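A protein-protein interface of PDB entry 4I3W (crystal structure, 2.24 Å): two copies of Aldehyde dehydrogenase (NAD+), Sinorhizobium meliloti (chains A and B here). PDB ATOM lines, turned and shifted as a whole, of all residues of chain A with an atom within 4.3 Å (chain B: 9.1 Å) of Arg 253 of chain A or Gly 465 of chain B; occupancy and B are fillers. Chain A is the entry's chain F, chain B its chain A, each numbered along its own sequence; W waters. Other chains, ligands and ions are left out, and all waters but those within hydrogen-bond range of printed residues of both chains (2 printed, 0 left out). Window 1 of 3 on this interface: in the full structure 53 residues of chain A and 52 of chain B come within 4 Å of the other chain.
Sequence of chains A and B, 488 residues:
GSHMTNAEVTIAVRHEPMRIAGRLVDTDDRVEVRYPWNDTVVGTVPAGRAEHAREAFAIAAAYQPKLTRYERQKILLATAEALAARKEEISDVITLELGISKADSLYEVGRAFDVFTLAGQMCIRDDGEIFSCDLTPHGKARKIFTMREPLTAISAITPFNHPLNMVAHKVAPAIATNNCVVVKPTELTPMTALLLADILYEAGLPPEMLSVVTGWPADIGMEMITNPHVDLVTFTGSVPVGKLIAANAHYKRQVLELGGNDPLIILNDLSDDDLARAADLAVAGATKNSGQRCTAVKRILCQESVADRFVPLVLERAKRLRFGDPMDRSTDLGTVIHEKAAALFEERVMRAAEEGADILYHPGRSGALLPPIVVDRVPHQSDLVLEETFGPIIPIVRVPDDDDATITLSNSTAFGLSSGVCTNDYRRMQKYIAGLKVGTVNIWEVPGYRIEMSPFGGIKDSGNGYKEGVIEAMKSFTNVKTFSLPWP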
ATOM      1  N   LEU A 151      -3.210   1.688   3.951  1.00  0.00           N
ATOM      2  CA  LEU A 151      -1.977   0.944   4.119  1.00  0.00           C
ATOM      3  C   LEU A 151      -1.080   1.697   5.100  1.00  0.00           C
ATOM      4  O   LEU A 151      -1.444   2.802   5.574  1.00  0.00           O
ATOM      5  CB  LEU A 151      -1.262   0.799   2.761  1.00  0.00           C
ATOM      6  CG  LEU A 151      -2.182   0.249   1.662  1.00  0.00           C
ATOM      7  CD1 LEU A 151      -1.462  -0.019   0.311  1.00  0.00           C
ATOM      8  CD2 LEU A 151      -2.918  -1.008   2.126  1.00  0.00           C
ATOM      9  N   ASP A 231       4.067  -0.605   1.832  1.00  0.00           N
ATOM     10  CA  ASP A 231       3.119  -1.707   1.572  1.00  0.00           C
ATOM     11  C   ASP A 231       2.893  -1.842   0.080  1.00  0.00           C
ATOM     12  O   ASP A 231       2.539  -2.912  -0.432  1.00  0.00           O
ATOM     13  CB  ASP A 231       1.773  -1.461   2.270  1.00  0.00           C
ATOM     14  CG  ASP A 231       1.809  -1.787   3.772  1.00  0.00           C
ATOM     15  OD1 ASP A 231       2.767  -2.469   4.210  1.00  0.00           O
ATOM     16  OD2 ASP A 231       0.866  -1.367   4.497  1.00  0.00           O
ATOM     17  N   LEU A 232       3.103  -0.737  -0.630  1.00  0.00           N
ATOM     18  CA  LEU A 232       2.769  -0.695  -2.058  1.00  0.00           C
ATOM     19  C   LEU A 232       3.672   0.277  -2.842  1.00  0.00           C
ATOM     20  O   LEU A 232       3.904   1.427  -2.433  1.00  0.00           O
ATOM     21  CB  LEU A 232       1.266  -0.335  -2.247  1.00  0.00           C
ATOM     22  CG  LEU A 232       0.698  -0.372  -3.675  1.00  0.00           C
ATOM     23  CD1 LEU A 232      -0.750  -0.780  -3.658  1.00  0.00           C
ATOM     24  CD2 LEU A 232       0.871   0.971  -4.399  1.00  0.00           C
ATOM     25  N   VAL A 233       4.157  -0.202  -3.973  1.00  0.00           N
ATOM     26  CA  VAL A 233       4.958   0.596  -4.866  1.00  0.00           C
ATOM     27  C   VAL A 233       4.112   0.845  -6.101  1.00  0.00           C
ATOM     28  O   VAL A 233       3.634  -0.108  -6.748  1.00  0.00           O
ATOM     29  CB  VAL A 233       6.237  -0.137  -5.302  1.00  0.00           C
ATOM     30  CG1 VAL A 233       7.010   0.719  -6.317  1.00  0.00           C
ATOM     31  CG2 VAL A 233       7.126  -0.469  -4.073  1.00  0.00           C
ATOM     32  N   LYS A 252       5.943  -6.928  -1.802  1.00  0.00           N
ATOM     33  CA  LYS A 252       5.236  -5.645  -1.741  1.00  0.00           C
ATOM     34  C   LYS A 252       4.238  -5.643  -2.875  1.00  0.00           C
ATOM     35  O   LYS A 252       4.522  -6.196  -3.946  1.00  0.00           O
ATOM     36  CB  LYS A 252       6.213  -4.479  -1.898  1.00  0.00           C
ATOM     37  CG  LYS A 252       7.208  -4.342  -0.735  1.00  0.00           C
ATOM     38  CD  LYS A 252       8.090  -3.135  -0.881  1.00  0.00           C
ATOM     39  CE  LYS A 252       9.114  -3.071   0.255  1.00  0.00           C
ATOM     40  NZ  LYS A 252       8.449  -3.066   1.586  1.00  0.00           N
ATOM     41  N   ARG A 253       3.052  -5.064  -2.673  1.00  0.00           N
ATOM     42  CA  ARG A 253       2.137  -4.935  -3.809  1.00  0.00           C
ATOM     43  C   ARG A 253       2.775  -3.963  -4.743  1.00  0.00           C
ATOM     44  O   ARG A 253       3.453  -3.018  -4.313  1.00  0.00           O
ATOM     45  CB  ARG A 253       0.787  -4.405  -3.403  1.00  0.00           C
ATOM     46  CG  ARG A 253       0.371  -4.923  -2.050  1.00  0.00           C
ATOM     47  CD  ARG A 253      -0.972  -5.563  -2.143  1.00  0.00           C
ATOM     48  NE  ARG A 253      -2.053  -4.584  -1.998  1.00  0.00           N
ATOM     49  CZ  ARG A 253      -2.551  -4.160  -0.836  1.00  0.00           C
ATOM     50  NH1 ARG A 253      -2.064  -4.590   0.338  1.00  0.00           N
ATOM     51  NH2 ARG A 253      -3.543  -3.282  -0.855  1.00  0.00           N
ATOM     52  N   GLN A 254       2.605  -4.221  -6.023  1.00  0.00           N
ATOM     53  CA  GLN A 254       3.255  -3.408  -7.058  1.00  0.00           C
ATOM     54  C   GLN A 254       2.233  -3.043  -8.122  1.00  0.00           C
ATOM     55  O   GLN A 254       1.463  -3.876  -8.575  1.00  0.00           O
ATOM     56  CB  GLN A 254       4.379  -4.183  -7.719  1.00  0.00           C
ATOM     57  CG  GLN A 254       5.548  -4.543  -6.808  1.00  0.00           C
ATOM     58  CD  GLN A 254       6.432  -5.621  -7.457  1.00  0.00           C
ATOM     59  OE1 GLN A 254       6.446  -5.757  -8.684  1.00  0.00           O
ATOM     60  NE2 GLN A 254       7.143  -6.408  -6.629  1.00  0.00           N
ATOM     61  N   SER A 476      -7.052  -0.075  -4.824  1.00  0.00           N
ATOM     62  CA  SER A 476      -5.712  -0.639  -4.806  1.00  0.00           C
ATOM     63  C   SER A 476      -4.898  -0.164  -3.596  1.00  0.00           C
ATOM     64  O   SER A 476      -4.059  -0.885  -3.033  1.00  0.00           O
ATOM     65  CB  SER A 476      -5.066  -0.130  -6.093  1.00  0.00           C
ATOM     66  OG  SER A 476      -4.089  -0.949  -6.570  1.00  0.00           O
ATOM     67  N   THR A 478      -5.930   0.302  -0.660  1.00  0.00           N
ATOM     68  CA  THR A 478      -6.578  -0.097   0.604  1.00  0.00           C
ATOM     69  C   THR A 478      -6.523  -1.585   0.818  1.00  0.00           C
ATOM     70  O   THR A 478      -6.208  -2.346  -0.096  1.00  0.00           O
ATOM     71  CB  THR A 478      -8.061   0.328   0.672  1.00  0.00           C
ATOM     72  OG1 THR A 478      -8.784  -0.330  -0.370  1.00  0.00           O
ATOM     73  CG2 THR A 478      -8.227   1.833   0.490  1.00  0.00           C
ATOM     74  N   ASN A 479      -6.800  -1.991   2.051  1.00  0.00           N
ATOM     75  CA  ASN A 479      -7.022  -3.385   2.370  1.00  0.00           C
ATOM     76  C   ASN A 479      -8.501  -3.530   2.672  1.00  0.00           C
ATOM     77  O   ASN A 479      -9.060  -2.744   3.436  1.00  0.00           O
ATOM     78  CB  ASN A 479      -6.226  -3.807   3.614  1.00  0.00           C
ATOM     79  CG  ASN A 479      -4.759  -3.944   3.346  1.00  0.00           C
ATOM     80  OD1 ASN A 479      -4.345  -4.501   2.317  1.00  0.00           O
ATOM     81  ND2 ASN A 479      -3.945  -3.443   4.263  1.00  0.00           N
ATOM     82  N   ALA B 246       7.673 -15.178  -3.779  1.00  0.00           N
ATOM     83  CA  ALA B 246       7.572 -13.754  -4.134  1.00  0.00           C
ATOM     84  C   ALA B 246       8.862 -13.221  -4.764  1.00  0.00           C
ATOM     85  O   ALA B 246       8.811 -12.398  -5.667  1.00  0.00           O
ATOM     86  CB  ALA B 246       7.191 -12.916  -2.918  1.00  0.00           C
ATOM     87  N   GLN B 254       0.838 -12.489  -8.257  1.00  0.00           N
ATOM     88  CA  GLN B 254       1.045 -13.465  -7.195  1.00  0.00           C
ATOM     89  C   GLN B 254      -0.079 -13.286  -6.202  1.00  0.00           C
ATOM     90  O   GLN B 254      -0.379 -12.165  -5.787  1.00  0.00           O
ATOM     91  CB  GLN B 254       2.367 -13.215  -6.470  1.00  0.00           C
ATOM     92  CG  GLN B 254       3.596 -13.327  -7.336  1.00  0.00           C
ATOM     93  CD  GLN B 254       4.828 -12.733  -6.669  1.00  0.00           C
ATOM     94  OE1 GLN B 254       4.866 -12.550  -5.468  1.00  0.00           O
ATOM     95  NE2 GLN B 254       5.832 -12.436  -7.458  1.00  0.00           N
ATOM     96  N   VAL B 255      -0.727 -14.382  -5.838  1.00  0.00           N
ATOM     97  CA  VAL B 255      -1.696 -14.358  -4.759  1.00  0.00           C
ATOM     98  C   VAL B 255      -1.154 -15.328  -3.732  1.00  0.00           C
ATOM     99  O   VAL B 255      -1.215 -16.549  -3.950  1.00  0.00           O
ATOM    100  CB  VAL B 255      -3.082 -14.799  -5.269  1.00  0.00           C
ATOM    101  CG1 VAL B 255      -4.085 -14.881  -4.147  1.00  0.00           C
ATOM    102  CG2 VAL B 255      -3.582 -13.829  -6.346  1.00  0.00           C
ATOM    103  N   LEU B 256      -0.550 -14.788  -2.667  1.00  0.00           N
ATOM    104  CA  LEU B 256       0.092 -15.618  -1.636  1.00  0.00           C
ATOM    105  C   LEU B 256      -0.669 -15.546  -0.306  1.00  0.00           C
ATOM    106  O   LEU B 256      -0.877 -14.470   0.258  1.00  0.00           O
ATOM    107  CB  LEU B 256       1.536 -15.146  -1.396  1.00  0.00           C
ATOM    108  CG  LEU B 256       2.290 -14.782  -2.670  1.00  0.00           C
ATOM    109  CD1 LEU B 256       3.682 -14.193  -2.369  1.00  0.00           C
ATOM    110  CD2 LEU B 256       2.382 -16.023  -3.580  1.00  0.00           C
ATOM    111  N   GLU B 257      -1.104 -16.696   0.175  1.00  0.00           N
ATOM    112  CA  GLU B 257      -1.717 -16.787   1.487  1.00  0.00           C
ATOM    113  C   GLU B 257      -0.784 -17.637   2.309  1.00  0.00           C
ATOM    114  O   GLU B 257      -0.442 -18.790   1.961  1.00  0.00           O
ATOM    115  CB  GLU B 257      -3.134 -17.392   1.478  1.00  0.00           C
ATOM    116  CG  GLU B 257      -4.174 -16.517   0.809  1.00  0.00           C
ATOM    117  CD  GLU B 257      -4.235 -15.095   1.379  1.00  0.00           C
ATOM    118  OE1 GLU B 257      -3.946 -14.890   2.608  1.00  0.00           O
ATOM    119  OE2 GLU B 257      -4.600 -14.184   0.583  1.00  0.00           O
ATOM    120  N   LEU B 258      -0.316 -17.017   3.371  1.00  0.00           N
ATOM    121  CA  LEU B 258       0.662 -17.625   4.210  1.00  0.00           C
ATOM    122  C   LEU B 258      -0.084 -17.949   5.505  1.00  0.00           C
ATOM    123  O   LEU B 258      -1.323 -17.984   5.530  1.00  0.00           O
ATOM    124  CB  LEU B 258       1.817 -16.655   4.391  1.00  0.00           C
ATOM    125  CG  LEU B 258       2.767 -16.448   3.192  1.00  0.00           C
ATOM    126  CD1 LEU B 258       2.244 -16.967   1.853  1.00  0.00           C
ATOM    127  CD2 LEU B 258       3.226 -14.995   3.023  1.00  0.00           C
ATOM    128  N   GLY B 416      -1.618 -11.492  10.605  1.00  0.00           N
ATOM    129  CA  GLY B 416      -2.848 -10.737  10.612  1.00  0.00           C
ATOM    130  C   GLY B 416      -3.805 -11.320   9.577  1.00  0.00           C
ATOM    131  O   GLY B 416      -3.922 -10.812   8.460  1.00  0.00           O
ATOM    132  N   PHE B 456     -11.451 -13.243   1.225  1.00  0.00           N
ATOM    133  CA  PHE B 456     -10.613 -13.878   2.221  1.00  0.00           C
ATOM    134  C   PHE B 456      -9.178 -13.557   1.940  1.00  0.00           C
ATOM    135  O   PHE B 456      -8.714 -13.732   0.803  1.00  0.00           O
ATOM    136  CB  PHE B 456     -10.759 -15.389   2.202  1.00  0.00           C
ATOM    137  CG  PHE B 456      -9.793 -16.095   3.113  1.00  0.00           C
ATOM    138  CD1 PHE B 456     -10.041 -16.193   4.482  1.00  0.00           C
ATOM    139  CD2 PHE B 456      -8.625 -16.651   2.610  1.00  0.00           C
ATOM    140  CE1 PHE B 456      -9.143 -16.857   5.321  1.00  0.00           C
ATOM    141  CE2 PHE B 456      -7.725 -17.288   3.441  1.00  0.00           C
ATOM    142  CZ  PHE B 456      -7.985 -17.390   4.794  1.00  0.00           C
ATOM    143  N   GLY B 457      -8.469 -13.096   2.968  1.00  0.00           N
ATOM    144  CA  GLY B 457      -7.037 -12.819   2.848  1.00  0.00           C
ATOM    145  C   GLY B 457      -6.518 -12.018   4.029  1.00  0.00           C
ATOM    146  O   GLY B 457      -7.272 -11.240   4.624  1.00  0.00           O
ATOM    147  N   GLY B 458      -5.244 -12.214   4.371  1.00  0.00           N
ATOM    148  CA  GLY B 458      -4.647 -11.442   5.451  1.00  0.00           C
ATOM    149  C   GLY B 458      -3.714 -10.328   5.019  1.00  0.00           C
ATOM    150  O   GLY B 458      -3.592  -9.987   3.829  1.00  0.00           O
ATOM    151  N   ILE B 459      -3.062  -9.737   6.010  1.00  0.00           N
ATOM    152  CA  ILE B 459      -2.081  -8.677   5.802  1.00  0.00           C
ATOM    153  C   ILE B 459      -0.843  -9.109   6.581  1.00  0.00           C
ATOM    154  O   ILE B 459      -0.801 -10.263   7.078  1.00  0.00           O
ATOM    155  CB  ILE B 459      -2.618  -7.339   6.318  1.00  0.00           C
ATOM    156  CG1 ILE B 459      -3.051  -7.464   7.777  1.00  0.00           C
ATOM    157  CG2 ILE B 459      -3.847  -6.889   5.484  1.00  0.00           C
ATOM    158  CD1 ILE B 459      -3.417  -6.156   8.411  1.00  0.00           C
ATOM    159  N   LYS B 460       0.140  -8.212   6.700  1.00  0.00           N
ATOM    160  CA  LYS B 460       1.392  -8.492   7.397  1.00  0.00           C
ATOM    161  C   LYS B 460       2.000  -9.758   6.813  1.00  0.00           C
ATOM    162  O   LYS B 460       2.011  -9.908   5.593  1.00  0.00           O
ATOM    163  CB  LYS B 460       1.184  -8.554   8.922  1.00  0.00           C
ATOM    164  CG  LYS B 460       0.703  -7.177   9.489  1.00  0.00           C
ATOM    165  CD  LYS B 460       0.065  -7.276  10.886  1.00  0.00           C
ATOM    166  CE  LYS B 460       1.089  -7.606  11.975  1.00  0.00           C
ATOM    167  NZ  LYS B 460       0.410  -7.758  13.280  1.00  0.00           N
ATOM    168  N   ASP B 461       2.476 -10.681   7.646  1.00  0.00           N
ATOM    169  CA  ASP B 461       3.051 -11.913   7.122  1.00  0.00           C
ATOM    170  C   ASP B 461       2.020 -12.975   6.687  1.00  0.00           C
ATOM    171  O   ASP B 461       2.427 -14.036   6.213  1.00  0.00           O
ATOM    172  CB  ASP B 461       4.018 -12.541   8.142  1.00  0.00           C
ATOM    173  CG  ASP B 461       5.438 -11.990   8.028  1.00  0.00           C
ATOM    174  OD1 ASP B 461       5.656 -11.086   7.205  1.00  0.00           O
ATOM    175  OD2 ASP B 461       6.340 -12.483   8.750  1.00  0.00           O
ATOM    176  N   SER B 462       0.719 -12.699   6.833  1.00  0.00           N
ATOM    177  CA  SER B 462      -0.330 -13.682   6.544  1.00  0.00           C
ATOM    178  C   SER B 462      -0.670 -13.731   5.063  1.00  0.00           C
ATOM    179  O   SER B 462      -1.262 -14.697   4.578  1.00  0.00           O
ATOM    180  CB  SER B 462      -1.623 -13.392   7.349  1.00  0.00           C
ATOM    181  OG  SER B 462      -1.426 -13.625   8.742  1.00  0.00           O
ATOM    182  N   GLY B 463      -0.307 -12.684   4.331  1.00  0.00           N
ATOM    183  CA  GLY B 463      -0.571 -12.658   2.911  1.00  0.00           C
ATOM    184  C   GLY B 463       0.011 -11.424   2.250  1.00  0.00           C
ATOM    185  O   GLY B 463       0.273 -10.411   2.905  1.00  0.00           O
ATOM    186  N   ASN B 464       0.189 -11.495   0.938  1.00  0.00           N
ATOM    187  CA  ASN B 464       0.757 -10.368   0.196  1.00  0.00           C
ATOM    188  C   ASN B 464      -0.259  -9.295  -0.162  1.00  0.00           C
ATOM    189  O   ASN B 464       0.081  -8.360  -0.873  1.00  0.00           O
ATOM    190  CB  ASN B 464       1.565 -10.831  -1.041  1.00  0.00           C
ATOM    191  CG  ASN B 464       0.690 -11.447  -2.145  1.00  0.00           C
ATOM    192  OD1 ASN B 464      -0.348 -12.048  -1.889  1.00  0.00           O
ATOM    193  ND2 ASN B 464       1.117 -11.279  -3.403  1.00  0.00           N
ATOM    194  N   GLY B 465      -1.502  -9.425   0.323  1.00  0.00           N
ATOM    195  CA  GLY B 465      -2.476  -8.334   0.262  1.00  0.00           C
ATOM    196  C   GLY B 465      -3.573  -8.425  -0.800  1.00  0.00           C
ATOM    197  O   GLY B 465      -4.276  -7.443  -1.068  1.00  0.00           O
ATOM    198  N   TYR B 466      -3.734  -9.591  -1.417  1.00  0.00           N
ATOM    199  CA  TYR B 466      -4.809  -9.795  -2.403  1.00  0.00           C
ATOM    200  C   TYR B 466      -5.854 -10.775  -1.857  1.00  0.00           C
ATOM    201  O   TYR B 466      -5.512 -11.745  -1.169  1.00  0.00           O
ATOM    202  CB  TYR B 466      -4.230 -10.299  -3.731  1.00  0.00           C
ATOM    203  CG  TYR B 466      -3.247  -9.335  -4.332  1.00  0.00           C
ATOM    204  CD1 TYR B 466      -3.685  -8.202  -5.013  1.00  0.00           C
ATOM    205  CD2 TYR B 466      -1.876  -9.529  -4.197  1.00  0.00           C
ATOM    206  CE1 TYR B 466      -2.768  -7.287  -5.572  1.00  0.00           C
ATOM    207  CE2 TYR B 466      -0.967  -8.631  -4.732  1.00  0.00           C
ATOM    208  CZ  TYR B 466      -1.429  -7.508  -5.430  1.00  0.00           C
ATOM    209  OH  TYR B 466      -0.554  -6.606  -5.975  1.00  0.00           O
ATOM    210  N   LYS B 467      -7.131 -10.498  -2.114  1.00  0.00           N
ATOM    211  CA  LYS B 467      -8.206 -11.345  -1.607  1.00  0.00           C
ATOM    212  C   LYS B 467      -8.424 -12.605  -2.435  1.00  0.00           C
ATOM    213  O   LYS B 467      -8.098 -12.650  -3.611  1.00  0.00           O
ATOM    214  CB  LYS B 467      -9.501 -10.567  -1.471  1.00  0.00           C
ATOM    215  CG  LYS B 467      -9.466  -9.467  -0.378  1.00  0.00           C
ATOM    216  CD  LYS B 467      -9.187 -10.066   0.996  1.00  0.00           C
ATOM    217  CE  LYS B 467      -9.177  -8.950   2.032  1.00  0.00           C
ATOM    218  NZ  LYS B 467      -9.297  -9.434   3.425  1.00  0.00           N
ATOM    219  N   GLU B 468      -8.945 -13.630  -1.771  1.00  0.00           N
ATOM    220  CA  GLU B 468      -9.220 -14.952  -2.341  1.00  0.00           C
ATOM    221  C   GLU B 468     -10.683 -15.238  -1.997  1.00  0.00           C
ATOM    222  O   GLU B 468     -11.445 -14.334  -1.612  1.00  0.00           O
ATOM    223  CB  GLU B 468      -8.374 -16.021  -1.607  1.00  0.00           C
ATOM    224  CG  GLU B 468      -7.210 -16.667  -2.341  1.00  0.00           C
ATOM    225  CD  GLU B 468      -6.793 -17.979  -1.666  1.00  0.00           C
ATOM    226  OE1 GLU B 468      -6.825 -18.032  -0.431  1.00  0.00           O
ATOM    227  OE2 GLU B 468      -6.502 -18.987  -2.361  1.00  0.00           O
ATOM    228  N   GLU B 472     -13.476 -13.381  -5.409  1.00  0.00           N
ATOM    229  CA  GLU B 472     -12.289 -12.538  -5.655  1.00  0.00           C
ATOM    230  C   GLU B 472     -11.268 -13.282  -6.504  1.00  0.00           C
ATOM    231  O   GLU B 472     -10.532 -12.678  -7.295  1.00  0.00           O
ATOM    232  CB  GLU B 472     -11.695 -12.045  -4.340  1.00  0.00           C
ATOM    233  CG  GLU B 472     -12.597 -11.015  -3.650  1.00  0.00           C
ATOM    234  CD  GLU B 472     -12.751  -9.717  -4.465  1.00  0.00           C
ATOM    235  OE1 GLU B 472     -11.826  -9.384  -5.260  1.00  0.00           O
ATOM    236  OE2 GLU B 472     -13.792  -9.011  -4.312  1.00  0.00           O
ATOM    237  N   SER B 476      -9.559 -12.100  -9.984  1.00  0.00           N
ATOM    238  CA  SER B 476      -8.107 -12.150  -9.968  1.00  0.00           C
ATOM    239  C   SER B 476      -7.521 -12.925 -11.162  1.00  0.00           C
ATOM    240  O   SER B 476      -6.426 -12.642 -11.662  1.00  0.00           O
ATOM    241  CB  SER B 476      -7.753 -12.918  -8.688  1.00  0.00           C
ATOM    242  OG  SER B 476      -6.648 -12.423  -8.064  1.00  0.00           O
HETATM  243  O   HOH W   1      -5.527  -6.471   1.401  1.00  0.00           O
HETATM  244  O   HOH W   2       2.104  -7.004  -6.666  1.00  0.00           O
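The backbone carbonyl oxygen (O) of Gln 254 of chain B is in hydrogen-bond range of the side-chain amide nitrogen (ND2) of Asn 464 of chain B, 3.0 Å away.
The side-chain amide oxygen (OD1) of Asn 464 of chain B sits at hydrogen-bond distance from the backbone NH (N) of Leu 256 of chain B, 2.9 Å away.
O of Asp 231 of chain A lies within hydrogen-bond range of N of Arg 253 of chain A.
O of Ser 476 of chain A is in hydrogen-bond range of NH2 of Arg 253 of chain A (3.3 Å).
NH2 of Arg 253 of chain A is in hydrogen-bond range of O of Thr 478 of chain A.
The guanidinium group (NH1) of Arg 253 of chain A is in hydrogen-bond range of the side-chain amide oxygen (OD1) of Asn 479 of chain A (3.0 Å).
Asn 464 of chain B touches Arg 253 of chain A.
Gly 465 of chain B touches Arg 253 of chain A.
Arg 253 of chain A touches Tyr 466 of chain B.
Gln 254 of chain A touches Tyr 466 of chain B (N to OH, 3.96 Å).
Asn 479 of chain A touches Ile 459 of chain B.
No residue of chain B comes within 4 Å of Leu 232 of chain A.
Lys 252 of chain A touches none of the printed residues of chain B.
Of chain B, only Asn 464 (3.2 Å), Gly 465 (3.7 Å) and Tyr 466 (3.6 Å) come within 4 Å of Arg 253 of chain A.
Printed residues of chain B within 4 Å of Asn 479 of chain A: Ile 459 (3.7 Å).
Of the printed residues of chain A, Ile 459 of chain B touches Asn 479.
Printed residues of chain A within 4 Å of Asn 464 of chain B: Arg 253.
Of chain A, only Arg 253 comes within 4 Å of Gly 465 of chain B.
The nearest residue of chain B that does not touch Arg 253 of chain A is Ile 459 of chain B (5.9 Å).
Hydrophobic or aromatic side chains of chain B that line the printed part of chain A: Ile 459 and Tyr 466.
Of the 10 printed residues of chain A, 3 touch a printed residue of chain B.
Among the printed residues, 5 pairs touch across the chains.
Among the printed residues, no Asp or Glu carboxylate lies within 4 Å of a Lys or Arg side-chain nitrogen of the other chain.
2 positions are printed for both chains.
Of the 5 pairs that touch across the chains among the printed residues, none has its exchanged pair printed and touching as well.
Water W1 bridges OD1 of Asn 479 of chain A (2.5 Å) and O of Gly 465 of chain B (2.9 Å).
Water W2 bridges OH of Tyr 466 of chain B (2.8 Å) and N of Gln 254 of chain A (2.9 Å).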
